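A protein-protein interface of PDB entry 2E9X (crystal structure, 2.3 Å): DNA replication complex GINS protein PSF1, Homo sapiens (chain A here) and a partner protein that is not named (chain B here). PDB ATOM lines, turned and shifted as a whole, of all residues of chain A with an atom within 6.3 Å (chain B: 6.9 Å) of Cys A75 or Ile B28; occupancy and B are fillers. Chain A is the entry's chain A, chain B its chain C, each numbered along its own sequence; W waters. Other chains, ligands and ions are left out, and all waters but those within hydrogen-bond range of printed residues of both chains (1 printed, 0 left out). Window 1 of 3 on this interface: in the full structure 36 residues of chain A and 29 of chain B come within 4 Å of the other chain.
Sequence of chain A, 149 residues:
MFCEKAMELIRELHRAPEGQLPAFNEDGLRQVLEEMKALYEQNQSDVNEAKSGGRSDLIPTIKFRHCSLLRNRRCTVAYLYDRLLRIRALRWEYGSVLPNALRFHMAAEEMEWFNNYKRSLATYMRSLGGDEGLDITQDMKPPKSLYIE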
ATOM      1  N   CYS A   3     -17.331 -11.711  10.055  1.00  0.00           N
ATOM      2  CA  CYS A   3     -17.515 -10.267   9.966  1.00  0.00           C
ATOM      3  C   CYS A   3     -18.347  -9.575  11.044  1.00  0.00           C
ATOM      4  O   CYS A   3     -18.683  -8.406  10.896  1.00  0.00           O
ATOM      5  CB  CYS A   3     -18.080  -9.935   8.588  1.00  0.00           C
ATOM      6  SG  CYS A   3     -17.203 -10.813   7.277  1.00  0.00           S
ATOM      7  N   ALA A   6     -16.006  -7.112  12.840  1.00  0.00           N
ATOM      8  CA  ALA A   6     -15.763  -5.940  12.012  1.00  0.00           C
ATOM      9  C   ALA A   6     -16.900  -4.932  12.190  1.00  0.00           C
ATOM     10  O   ALA A   6     -16.665  -3.726  12.220  1.00  0.00           O
ATOM     11  CB  ALA A   6     -15.641  -6.351  10.556  1.00  0.00           C
ATOM     12  N   MET A   7     -18.128  -5.431  12.313  1.00  0.00           N
ATOM     13  CA  MET A   7     -19.287  -4.563  12.491  1.00  0.00           C
ATOM     14  C   MET A   7     -19.252  -3.793  13.801  1.00  0.00           C
ATOM     15  O   MET A   7     -19.846  -2.718  13.905  1.00  0.00           O
ATOM     16  CB  MET A   7     -20.584  -5.367  12.419  1.00  0.00           C
ATOM     17  CG  MET A   7     -20.988  -5.732  11.012  1.00  0.00           C
ATOM     18  SD  MET A   7     -21.053  -4.265   9.961  1.00  0.00           S
ATOM     19  CE  MET A   7     -22.443  -3.383  10.724  1.00  0.00           C
ATOM     20  N   LEU A   9     -16.630  -2.455  15.059  1.00  0.00           N
ATOM     21  CA  LEU A   9     -15.791  -1.299  14.775  1.00  0.00           C
ATOM     22  C   LEU A   9     -16.647  -0.191  14.177  1.00  0.00           C
ATOM     23  O   LEU A   9     -16.609   0.956  14.628  1.00  0.00           O
ATOM     24  CB  LEU A   9     -14.680  -1.662  13.777  1.00  0.00           C
ATOM     25  CG  LEU A   9     -13.535  -2.563  14.239  1.00  0.00           C
ATOM     26  CD1 LEU A   9     -12.604  -2.862  13.066  1.00  0.00           C
ATOM     27  CD2 LEU A   9     -12.765  -1.878  15.354  1.00  0.00           C
ATOM     28  N   ILE A  10     -17.419  -0.553  13.154  1.00  0.00           N
ATOM     29  CA  ILE A  10     -18.280   0.391  12.447  1.00  0.00           C
ATOM     30  C   ILE A  10     -19.326   1.038  13.347  1.00  0.00           C
ATOM     31  O   ILE A  10     -19.486   2.264  13.331  1.00  0.00           O
ATOM     32  CB  ILE A  10     -18.998  -0.297  11.260  1.00  0.00           C
ATOM     33  CG1 ILE A  10     -17.968  -0.969  10.338  1.00  0.00           C
ATOM     34  CG2 ILE A  10     -19.821   0.717  10.489  1.00  0.00           C
ATOM     35  CD1 ILE A  10     -16.968  -0.010   9.704  1.00  0.00           C
ATOM     36  N   LEU A  70     -13.406  -9.930   1.779  1.00  0.00           N
ATOM     37  CA  LEU A  70     -13.574  -8.607   1.190  1.00  0.00           C
ATOM     38  C   LEU A  70     -14.405  -7.712   2.107  1.00  0.00           C
ATOM     39  O   LEU A  70     -14.198  -6.502   2.153  1.00  0.00           O
ATOM     40  CB  LEU A  70     -14.248  -8.716  -0.181  1.00  0.00           C
ATOM     41  CG  LEU A  70     -13.424  -9.363  -1.303  1.00  0.00           C
ATOM     42  CD1 LEU A  70     -14.286  -9.475  -2.557  1.00  0.00           C
ATOM     43  CD2 LEU A  70     -12.176  -8.519  -1.594  1.00  0.00           C
ATOM     44  N   ARG A  71     -15.344  -8.313   2.830  1.00  0.00           N
ATOM     45  CA  ARG A  71     -16.184  -7.567   3.758  1.00  0.00           C
ATOM     46  C   ARG A  71     -15.340  -7.104   4.949  1.00  0.00           C
ATOM     47  O   ARG A  71     -15.390  -5.932   5.333  1.00  0.00           O
ATOM     48  CB  ARG A  71     -17.344  -8.440   4.238  1.00  0.00           C
ATOM     49  CG  ARG A  71     -18.204  -7.836   5.346  1.00  0.00           C
ATOM     50  CD  ARG A  71     -19.029  -6.623   4.896  1.00  0.00           C
ATOM     51  NE  ARG A  71     -19.967  -6.218   5.944  1.00  0.00           N
ATOM     52  CZ  ARG A  71     -20.881  -5.261   5.815  1.00  0.00           C
ATOM     53  NH1 ARG A  71     -20.996  -4.589   4.679  1.00  0.00           N
ATOM     54  NH2 ARG A  71     -21.692  -4.982   6.828  1.00  0.00           N
ATOM     55  N   ASN A  72     -14.566  -8.021   5.529  1.00  0.00           N
ATOM     56  CA  ASN A  72     -13.711  -7.669   6.659  1.00  0.00           C
ATOM     57  C   ASN A  72     -12.788  -6.532   6.258  1.00  0.00           C
ATOM     58  O   ASN A  72     -12.581  -5.596   7.029  1.00  0.00           O
ATOM     59  CB  ASN A  72     -12.868  -8.863   7.124  1.00  0.00           C
ATOM     60  CG  ASN A  72     -13.598  -9.741   8.120  1.00  0.00           C
ATOM     61  OD1 ASN A  72     -14.161  -9.253   9.105  1.00  0.00           O
ATOM     62  ND2 ASN A  72     -13.584 -11.043   7.879  1.00  0.00           N
ATOM     63  N   ARG A  73     -12.244  -6.607   5.046  1.00  0.00           N
ATOM     64  CA  ARG A  73     -11.339  -5.572   4.569  1.00  0.00           C
ATOM     65  C   ARG A  73     -12.056  -4.237   4.376  1.00  0.00           C
ATOM     66  O   ARG A  73     -11.518  -3.184   4.724  1.00  0.00           O
ATOM     67  CB  ARG A  73     -10.676  -5.987   3.252  1.00  0.00           C
ATOM     68  CG  ARG A  73      -9.591  -5.009   2.816  1.00  0.00           C
ATOM     69  CD  ARG A  73      -8.898  -5.438   1.539  1.00  0.00           C
ATOM     70  NE  ARG A  73      -9.737  -5.245   0.365  1.00  0.00           N
ATOM     71  CZ  ARG A  73      -9.316  -5.420  -0.883  1.00  0.00           C
ATOM     72  NH1 ARG A  73      -8.063  -5.791  -1.113  1.00  0.00           N
ATOM     73  NH2 ARG A  73     -10.144  -5.225  -1.901  1.00  0.00           N
ATOM     74  N   ARG A  74     -13.258  -4.278   3.813  1.00  0.00           N
ATOM     75  CA  ARG A  74     -14.028  -3.059   3.601  1.00  0.00           C
ATOM     76  C   ARG A  74     -14.296  -2.355   4.936  1.00  0.00           C
ATOM     77  O   ARG A  74     -14.114  -1.145   5.053  1.00  0.00           O
ATOM     78  CB  ARG A  74     -15.366  -3.371   2.918  1.00  0.00           C
ATOM     79  CG  ARG A  74     -16.187  -2.127   2.602  1.00  0.00           C
ATOM     80  CD  ARG A  74     -17.635  -2.448   2.255  1.00  0.00           C
ATOM     81  NE  ARG A  74     -18.392  -1.234   1.956  1.00  0.00           N
ATOM     82  CZ  ARG A  74     -19.714  -1.191   1.787  1.00  0.00           C
ATOM     83  NH1 ARG A  74     -20.439  -2.298   1.891  1.00  0.00           N
ATOM     84  NH2 ARG A  74     -20.311  -0.038   1.504  1.00  0.00           N
ATOM     85  N   CYS A  75     -14.727  -3.113   5.942  1.00  0.00           N
ATOM     86  CA  CYS A  75     -15.016  -2.524   7.251  1.00  0.00           C
ATOM     87  C   CYS A  75     -13.763  -1.933   7.886  1.00  0.00           C
ATOM     88  O   CYS A  75     -13.804  -0.858   8.484  1.00  0.00           O
ATOM     89  CB  CYS A  75     -15.615  -3.569   8.198  1.00  0.00           C
ATOM     90  SG  CYS A  75     -17.268  -4.148   7.727  1.00  0.00           S
ATOM     91  N   THR A  76     -12.654  -2.646   7.749  1.00  0.00           N
ATOM     92  CA  THR A  76     -11.388  -2.214   8.308  1.00  0.00           C
ATOM     93  C   THR A  76     -10.955  -0.878   7.735  1.00  0.00           C
ATOM     94  O   THR A  76     -10.639   0.057   8.480  1.00  0.00           O
ATOM     95  CB  THR A  76     -10.293  -3.264   8.037  1.00  0.00           C
ATOM     96  OG1 THR A  76     -10.596  -4.449   8.779  1.00  0.00           O
ATOM     97  CG2 THR A  76      -8.909  -2.738   8.441  1.00  0.00           C
ATOM     98  N   VAL A  77     -10.944  -0.789   6.411  1.00  0.00           N
ATOM     99  CA  VAL A  77     -10.537   0.434   5.739  1.00  0.00           C
ATOM    100  C   VAL A  77     -11.500   1.582   6.023  1.00  0.00           C
ATOM    101  O   VAL A  77     -11.064   2.709   6.256  1.00  0.00           O
ATOM    102  CB  VAL A  77     -10.420   0.218   4.205  1.00  0.00           C
ATOM    103  CG1 VAL A  77      -9.969   1.499   3.530  1.00  0.00           C
ATOM    104  CG2 VAL A  77      -9.423  -0.906   3.913  1.00  0.00           C
ATOM    105  N   ALA A  78     -12.804   1.306   6.005  1.00  0.00           N
ATOM    106  CA  ALA A  78     -13.801   2.345   6.275  1.00  0.00           C
ATOM    107  C   ALA A  78     -13.617   2.907   7.693  1.00  0.00           C
ATOM    108  O   ALA A  78     -13.658   4.120   7.911  1.00  0.00           O
ATOM    109  CB  ALA A  78     -15.217   1.779   6.109  1.00  0.00           C
ATOM    110  N   TYR A  79     -13.418   2.008   8.649  1.00  0.00           N
ATOM    111  CA  TYR A  79     -13.203   2.379  10.047  1.00  0.00           C
ATOM    112  C   TYR A  79     -11.977   3.293  10.165  1.00  0.00           C
ATOM    113  O   TYR A  79     -12.072   4.425  10.637  1.00  0.00           O
ATOM    114  CB  TYR A  79     -12.981   1.113  10.878  1.00  0.00           C
ATOM    115  CG  TYR A  79     -12.505   1.358  12.284  1.00  0.00           C
ATOM    116  CD1 TYR A  79     -13.387   1.776  13.289  1.00  0.00           C
ATOM    117  CD2 TYR A  79     -11.162   1.181  12.616  1.00  0.00           C
ATOM    118  CE1 TYR A  79     -12.934   2.009  14.590  1.00  0.00           C
ATOM    119  CE2 TYR A  79     -10.703   1.412  13.895  1.00  0.00           C
ATOM    120  CZ  TYR A  79     -11.589   1.827  14.882  1.00  0.00           C
ATOM    121  OH  TYR A  79     -11.100   2.065  16.147  1.00  0.00           O
ATOM    122  N   LEU A  80     -10.832   2.797   9.710  1.00  0.00           N
ATOM    123  CA  LEU A  80      -9.589   3.549   9.770  1.00  0.00           C
ATOM    124  C   LEU A  80      -9.654   4.876   9.021  1.00  0.00           C
ATOM    125  O   LEU A  80      -9.107   5.883   9.484  1.00  0.00           O
ATOM    126  CB  LEU A  80      -8.440   2.699   9.218  1.00  0.00           C
ATOM    127  CG  LEU A  80      -8.136   1.395   9.973  1.00  0.00           C
ATOM    128  CD1 LEU A  80      -7.198   0.508   9.137  1.00  0.00           C
ATOM    129  CD2 LEU A  80      -7.512   1.717  11.329  1.00  0.00           C
ATOM    130  N   GLU B  20     -23.354   1.043  -3.569  1.00  0.00           N
ATOM    131  CA  GLU B  20     -23.195   1.753  -2.314  1.00  0.00           C
ATOM    132  C   GLU B  20     -21.753   2.270  -2.249  1.00  0.00           C
ATOM    133  O   GLU B  20     -20.888   1.810  -3.004  1.00  0.00           O
ATOM    134  CB  GLU B  20     -23.553   0.827  -1.129  1.00  0.00           C
ATOM    135  CG  GLU B  20     -22.665  -0.383  -0.906  1.00  0.00           C
ATOM    136  CD  GLU B  20     -23.239  -1.379   0.122  1.00  0.00           C
ATOM    137  OE1 GLU B  20     -24.109  -2.203  -0.242  1.00  0.00           O
ATOM    138  OE2 GLU B  20     -22.821  -1.343   1.299  1.00  0.00           O
ATOM    139  N   ASN B  21     -21.497   3.259  -1.399  1.00  0.00           N
ATOM    140  CA  ASN B  21     -20.146   3.788  -1.289  1.00  0.00           C
ATOM    141  C   ASN B  21     -19.302   2.899  -0.391  1.00  0.00           C
ATOM    142  O   ASN B  21     -19.661   2.610   0.756  1.00  0.00           O
ATOM    143  CB  ASN B  21     -20.152   5.241  -0.777  1.00  0.00           C
ATOM    144  CG  ASN B  21     -20.400   6.248  -1.892  1.00  0.00           C
ATOM    145  OD1 ASN B  21     -19.987   6.034  -3.035  1.00  0.00           O
ATOM    146  ND2 ASN B  21     -21.059   7.355  -1.566  1.00  0.00           N
ATOM    147  N   PHE B  22     -18.173   2.461  -0.939  1.00  0.00           N
ATOM    148  CA  PHE B  22     -17.248   1.579  -0.240  1.00  0.00           C
ATOM    149  C   PHE B  22     -16.915   2.016   1.192  1.00  0.00           C
ATOM    150  O   PHE B  22     -16.966   1.212   2.120  1.00  0.00           O
ATOM    151  CB  PHE B  22     -15.954   1.459  -1.049  1.00  0.00           C
ATOM    152  CG  PHE B  22     -15.031   0.370  -0.570  1.00  0.00           C
ATOM    153  CD1 PHE B  22     -15.335  -0.970  -0.798  1.00  0.00           C
ATOM    154  CD2 PHE B  22     -13.839   0.686   0.081  1.00  0.00           C
ATOM    155  CE1 PHE B  22     -14.463  -1.987  -0.388  1.00  0.00           C
ATOM    156  CE2 PHE B  22     -12.959  -0.322   0.495  1.00  0.00           C
ATOM    157  CZ  PHE B  22     -13.273  -1.661   0.258  1.00  0.00           C
ATOM    158  N   LEU B  23     -16.595   3.293   1.363  1.00  0.00           N
ATOM    159  CA  LEU B  23     -16.206   3.826   2.671  1.00  0.00           C
ATOM    160  C   LEU B  23     -17.332   4.407   3.518  1.00  0.00           C
ATOM    161  O   LEU B  23     -17.077   4.950   4.593  1.00  0.00           O
ATOM    162  CB  LEU B  23     -15.128   4.899   2.485  1.00  0.00           C
ATOM    163  CG  LEU B  23     -13.899   4.463   1.674  1.00  0.00           C
ATOM    164  CD1 LEU B  23     -13.012   5.666   1.410  1.00  0.00           C
ATOM    165  CD2 LEU B  23     -13.137   3.375   2.427  1.00  0.00           C
ATOM    166  N   SER B  24     -18.566   4.302   3.039  1.00  0.00           N
ATOM    167  CA  SER B  24     -19.709   4.838   3.770  1.00  0.00           C
ATOM    168  C   SER B  24     -20.068   3.957   4.960  1.00  0.00           C
ATOM    169  O   SER B  24     -20.461   2.800   4.790  1.00  0.00           O
ATOM    170  CB  SER B  24     -20.920   4.982   2.830  1.00  0.00           C
ATOM    171  OG  SER B  24     -22.146   5.020   3.549  1.00  0.00           O
ATOM    172  N   LEU B  25     -19.934   4.501   6.165  1.00  0.00           N
ATOM    173  CA  LEU B  25     -20.264   3.731   7.358  1.00  0.00           C
ATOM    174  C   LEU B  25     -21.739   3.355   7.336  1.00  0.00           C
ATOM    175  O   LEU B  25     -22.113   2.243   7.710  1.00  0.00           O
ATOM    176  CB  LEU B  25     -19.957   4.533   8.629  1.00  0.00           C
ATOM    177  CG  LEU B  25     -18.489   4.909   8.862  1.00  0.00           C
ATOM    178  CD1 LEU B  25     -18.353   5.572  10.226  1.00  0.00           C
ATOM    179  CD2 LEU B  25     -17.605   3.663   8.798  1.00  0.00           C
ATOM    180  N   ASP B  26     -22.576   4.282   6.891  1.00  0.00           N
ATOM    181  CA  ASP B  26     -24.006   4.024   6.840  1.00  0.00           C
ATOM    182  C   ASP B  26     -24.379   2.901   5.872  1.00  0.00           C
ATOM    183  O   ASP B  26     -25.287   2.122   6.160  1.00  0.00           O
ATOM    184  CB  ASP B  26     -24.769   5.296   6.470  1.00  0.00           C
ATOM    185  CG  ASP B  26     -26.265   5.134   6.623  1.00  0.00           C
ATOM    186  OD1 ASP B  26     -26.707   4.745   7.733  1.00  0.00           O
ATOM    187  OD2 ASP B  26     -27.003   5.394   5.643  1.00  0.00           O
ATOM    188  N   ASP B  27     -23.706   2.826   4.723  1.00  0.00           N
ATOM    189  CA  ASP B  27     -24.003   1.763   3.768  1.00  0.00           C
ATOM    190  C   ASP B  27     -23.533   0.426   4.330  1.00  0.00           C
ATOM    191  O   ASP B  27     -24.162  -0.605   4.109  1.00  0.00           O
ATOM    192  CB  ASP B  27     -23.343   2.027   2.403  1.00  0.00           C
ATOM    193  CG  ASP B  27     -23.983   3.185   1.668  1.00  0.00           C
ATOM    194  OD1 ASP B  27     -25.130   3.557   2.016  1.00  0.00           O
ATOM    195  OD2 ASP B  27     -23.349   3.725   0.738  1.00  0.00           O
ATOM    196  N   ILE B  28     -22.433   0.446   5.075  1.00  0.00           N
ATOM    197  CA  ILE B  28     -21.927  -0.776   5.678  1.00  0.00           C
ATOM    198  C   ILE B  28     -22.916  -1.302   6.721  1.00  0.00           C
ATOM    199  O   ILE B  28     -23.096  -2.515   6.857  1.00  0.00           O
ATOM    200  CB  ILE B  28     -20.554  -0.547   6.335  1.00  0.00           C
ATOM    201  CG1 ILE B  28     -19.505  -0.304   5.251  1.00  0.00           C
ATOM    202  CG2 ILE B  28     -20.171  -1.747   7.184  1.00  0.00           C
ATOM    203  CD1 ILE B  28     -18.140   0.012   5.788  1.00  0.00           C
ATOM    204  N   LEU B  29     -23.556  -0.395   7.452  1.00  0.00           N
ATOM    205  CA  LEU B  29     -24.536  -0.793   8.463  1.00  0.00           C
ATOM    206  C   LEU B  29     -25.790  -1.282   7.740  1.00  0.00           C
ATOM    207  O   LEU B  29     -26.450  -2.217   8.172  1.00  0.00           O
ATOM    208  CB  LEU B  29     -24.893   0.394   9.365  1.00  0.00           C
ATOM    209  CG  LEU B  29     -23.829   0.860  10.364  1.00  0.00           C
ATOM    210  CD1 LEU B  29     -24.213   2.225  10.928  1.00  0.00           C
ATOM    211  CD2 LEU B  29     -23.698  -0.168  11.485  1.00  0.00           C
ATOM    212  N   MET B  30     -26.114  -0.637   6.629  1.00  0.00           N
ATOM    213  CA  MET B  30     -27.273  -1.020   5.845  1.00  0.00           C
ATOM    214  C   MET B  30     -27.118  -2.434   5.252  1.00  0.00           C
ATOM    215  O   MET B  30     -27.998  -3.283   5.418  1.00  0.00           O
ATOM    216  CB  MET B  30     -27.488   0.006   4.733  1.00  0.00           C
ATOM    217  CG  MET B  30     -28.634  -0.306   3.778  1.00  0.00           C
ATOM    218  SD  MET B  30     -28.218  -1.560   2.557  1.00  0.00           S
ATOM    219  CE  MET B  30     -27.223  -0.623   1.446  1.00  0.00           C
ATOM    220  N   SER B  31     -25.995  -2.691   4.585  1.00  0.00           N
ATOM    221  CA  SER B  31     -25.769  -3.996   3.969  1.00  0.00           C
ATOM    222  C   SER B  31     -25.513  -5.121   4.965  1.00  0.00           C
ATOM    223  O   SER B  31     -25.210  -6.245   4.576  1.00  0.00           O
ATOM    224  CB  SER B  31     -24.624  -3.921   2.955  1.00  0.00           C
ATOM    225  OG  SER B  31     -23.461  -3.330   3.508  1.00  0.00           O
ATOM    226  N   HIS B  32     -25.638  -4.816   6.253  1.00  0.00           N
ATOM    227  CA  HIS B  32     -25.448  -5.823   7.288  1.00  0.00           C
ATOM    228  C   HIS B  32     -26.804  -6.446   7.597  1.00  0.00           C
ATOM    229  O   HIS B  32     -26.884  -7.574   8.081  1.00  0.00           O
ATOM    230  CB  HIS B  32     -24.889  -5.186   8.560  1.00  0.00           C
ATOM    231  CG  HIS B  32     -24.886  -6.106   9.745  1.00  0.00           C
ATOM    232  ND1 HIS B  32     -23.972  -7.126   9.896  1.00  0.00           N
ATOM    233  CD2 HIS B  32     -25.693  -6.161  10.832  1.00  0.00           C
ATOM    234  CE1 HIS B  32     -24.212  -7.769  11.025  1.00  0.00           C
ATOM    235  NE2 HIS B  32     -25.252  -7.202  11.612  1.00  0.00           N
ATOM    236  N   GLU B  33     -27.864  -5.696   7.319  1.00  0.00           N
ATOM    237  CA  GLU B  33     -29.229  -6.144   7.565  1.00  0.00           C
ATOM    238  C   GLU B  33     -29.515  -7.439   6.801  1.00  0.00           C
ATOM    239  O   GLU B  33     -29.088  -7.607   5.656  1.00  0.00           O
ATOM    240  CB  GLU B  33     -30.195  -5.020   7.176  1.00  0.00           C
ATOM    241  CG  GLU B  33     -29.799  -3.700   7.844  1.00  0.00           C
ATOM    242  CD  GLU B  33     -30.590  -2.494   7.372  1.00  0.00           C
ATOM    243  OE1 GLU B  33     -30.946  -2.425   6.176  1.00  0.00           O
ATOM    244  OE2 GLU B  33     -30.833  -1.594   8.203  1.00  0.00           O
ATOM    245  N   TRP B  74     -24.781  -8.027   2.175  1.00  0.00           N
ATOM    246  CA  TRP B  74     -23.488  -8.096   1.503  1.00  0.00           C
ATOM    247  C   TRP B  74     -23.113  -9.515   1.077  1.00  0.00           C
ATOM    248  O   TRP B  74     -22.582  -9.714  -0.014  1.00  0.00           O
ATOM    249  CB  TRP B  74     -22.364  -7.498   2.372  1.00  0.00           C
ATOM    250  CG  TRP B  74     -22.134  -8.194   3.675  1.00  0.00           C
ATOM    251  CD1 TRP B  74     -22.680  -7.877   4.883  1.00  0.00           C
ATOM    252  CD2 TRP B  74     -21.310  -9.343   3.896  1.00  0.00           C
ATOM    253  NE1 TRP B  74     -22.247  -8.757   5.845  1.00  0.00           N
ATOM    254  CE2 TRP B  74     -21.405  -9.668   5.266  1.00  0.00           C
ATOM    255  CE3 TRP B  74     -20.500 -10.133   3.066  1.00  0.00           C
ATOM    256  CZ2 TRP B  74     -20.721 -10.753   5.830  1.00  0.00           C
ATOM    257  CZ3 TRP B  74     -19.819 -11.209   3.624  1.00  0.00           C
ATOM    258  CH2 TRP B  74     -19.934 -11.509   4.996  1.00  0.00           C
HETATM  259  O   HOH W   1     -15.075   5.955   6.116  1.00  0.00           O
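Water W1 lies within hydrogen-bond range of the backbone carbonyl oxygen of Leu B23 (2.7 Å) and the backbone carbonyl oxygen of Ala A78 (2.9 Å).
O of Phe B22 is in hydrogen-bond range of NE of Arg A74, 2.8 Å away. NH1 of Arg A74 lies within salt-bridge range of OE2 of Glu B20 (2.6 Å). The guanidinium group (NE) of Arg A71 lies close to the indole nitrogen (NE1) of Trp B74 (3.4 Å). NH2 of Arg A74 lies within hydrogen-bond range of O of Asn B21, at 2.8 Å. NH1 of Arg A71 lies within hydrogen-bond range of OG of Ser B31, at 3.0 Å. The guanidinium group of Arg A71 is in hydrogen-bond range of the backbone carbonyl oxygen of Ile B28 (2.8 Å).
Of the 16 printed residues of chain A, 8 touch a printed residue of chain B. Hydrophobic or aromatic side chains of chain A that line the printed part of chain B: Met A7, Ile A10, Val A77 and Ala A78. Of the 15 printed residues of chain B, 11 touch a printed residue of chain A. Hydrophobic or aromatic side chains of chain B within 4 Å of the printed part of chain A: Phe B22, Leu B23, Leu B25, Ile B28, Leu B29, His B32 and Trp B74.
Cys A3 touches Trp B74. CE of Met A7 touches CD2 of Leu B29, at 3.5 Å. CG of Met A7 touches ND1 of His B32, 3.5 Å away. Ile A10 touches Leu B25. NH2 of Arg A71 touches CB of His B32 (3.6 Å). Arg A74 touches Asp B27 (NH2 to CB, 3.8 Å). CZ of Arg A74 touches CG1 of Ile B28, 3.6 Å away. Ser B31 touches Arg A74. CG1 of Val A77 touches CD2 of Leu B23, 3.8 Å away. CB of Ala A78 touches CD1 of Ile B28, at 3.4 Å.
Cys A75 touches one residue of chain B. Of chain A, only Met A7, Ile A10, Arg A71, Arg A74, Cys A75 and Ala A78 come within 4 Å of Ile B28. Of the printed residues of chain A, Phe B22 touches Arg A74. Of the printed residues of chain B, Val A77 touches Leu B23. Of the printed residues of chain A, Leu B23 touches Val A77 and Ala A78. The nearest residue of chain A that does not touch Ile B28 is Tyr A79 (5.9 Å).
The backbone NH (N) of Asn B21 lies within hydrogen-bond range of the side-chain carboxylate (OD2) of Asp B27, 2.9 Å away. The backbone carbonyl oxygen of Asp B27 sits at hydrogen-bond distance from the side-chain hydroxyl of Ser B31. The backbone carbonyl oxygen (O) of Arg A71 is in hydrogen-bond range of the side-chain sulfur (SG) of Cys A75, 3.5 Å away. The backbone carbonyl oxygen of Ile B28 is in hydrogen-bond range of the side-chain hydroxyl of Ser B31. The backbone NH (N) of Trp B74 lies within hydrogen-bond range of the backbone carbonyl oxygen (O) of Ser B31 (3.0 Å). The guanidinium group (NH2) of Arg A71 sits at hydrogen-bond distance from the side-chain sulfur (SD) of Met A7 (3.3 Å).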
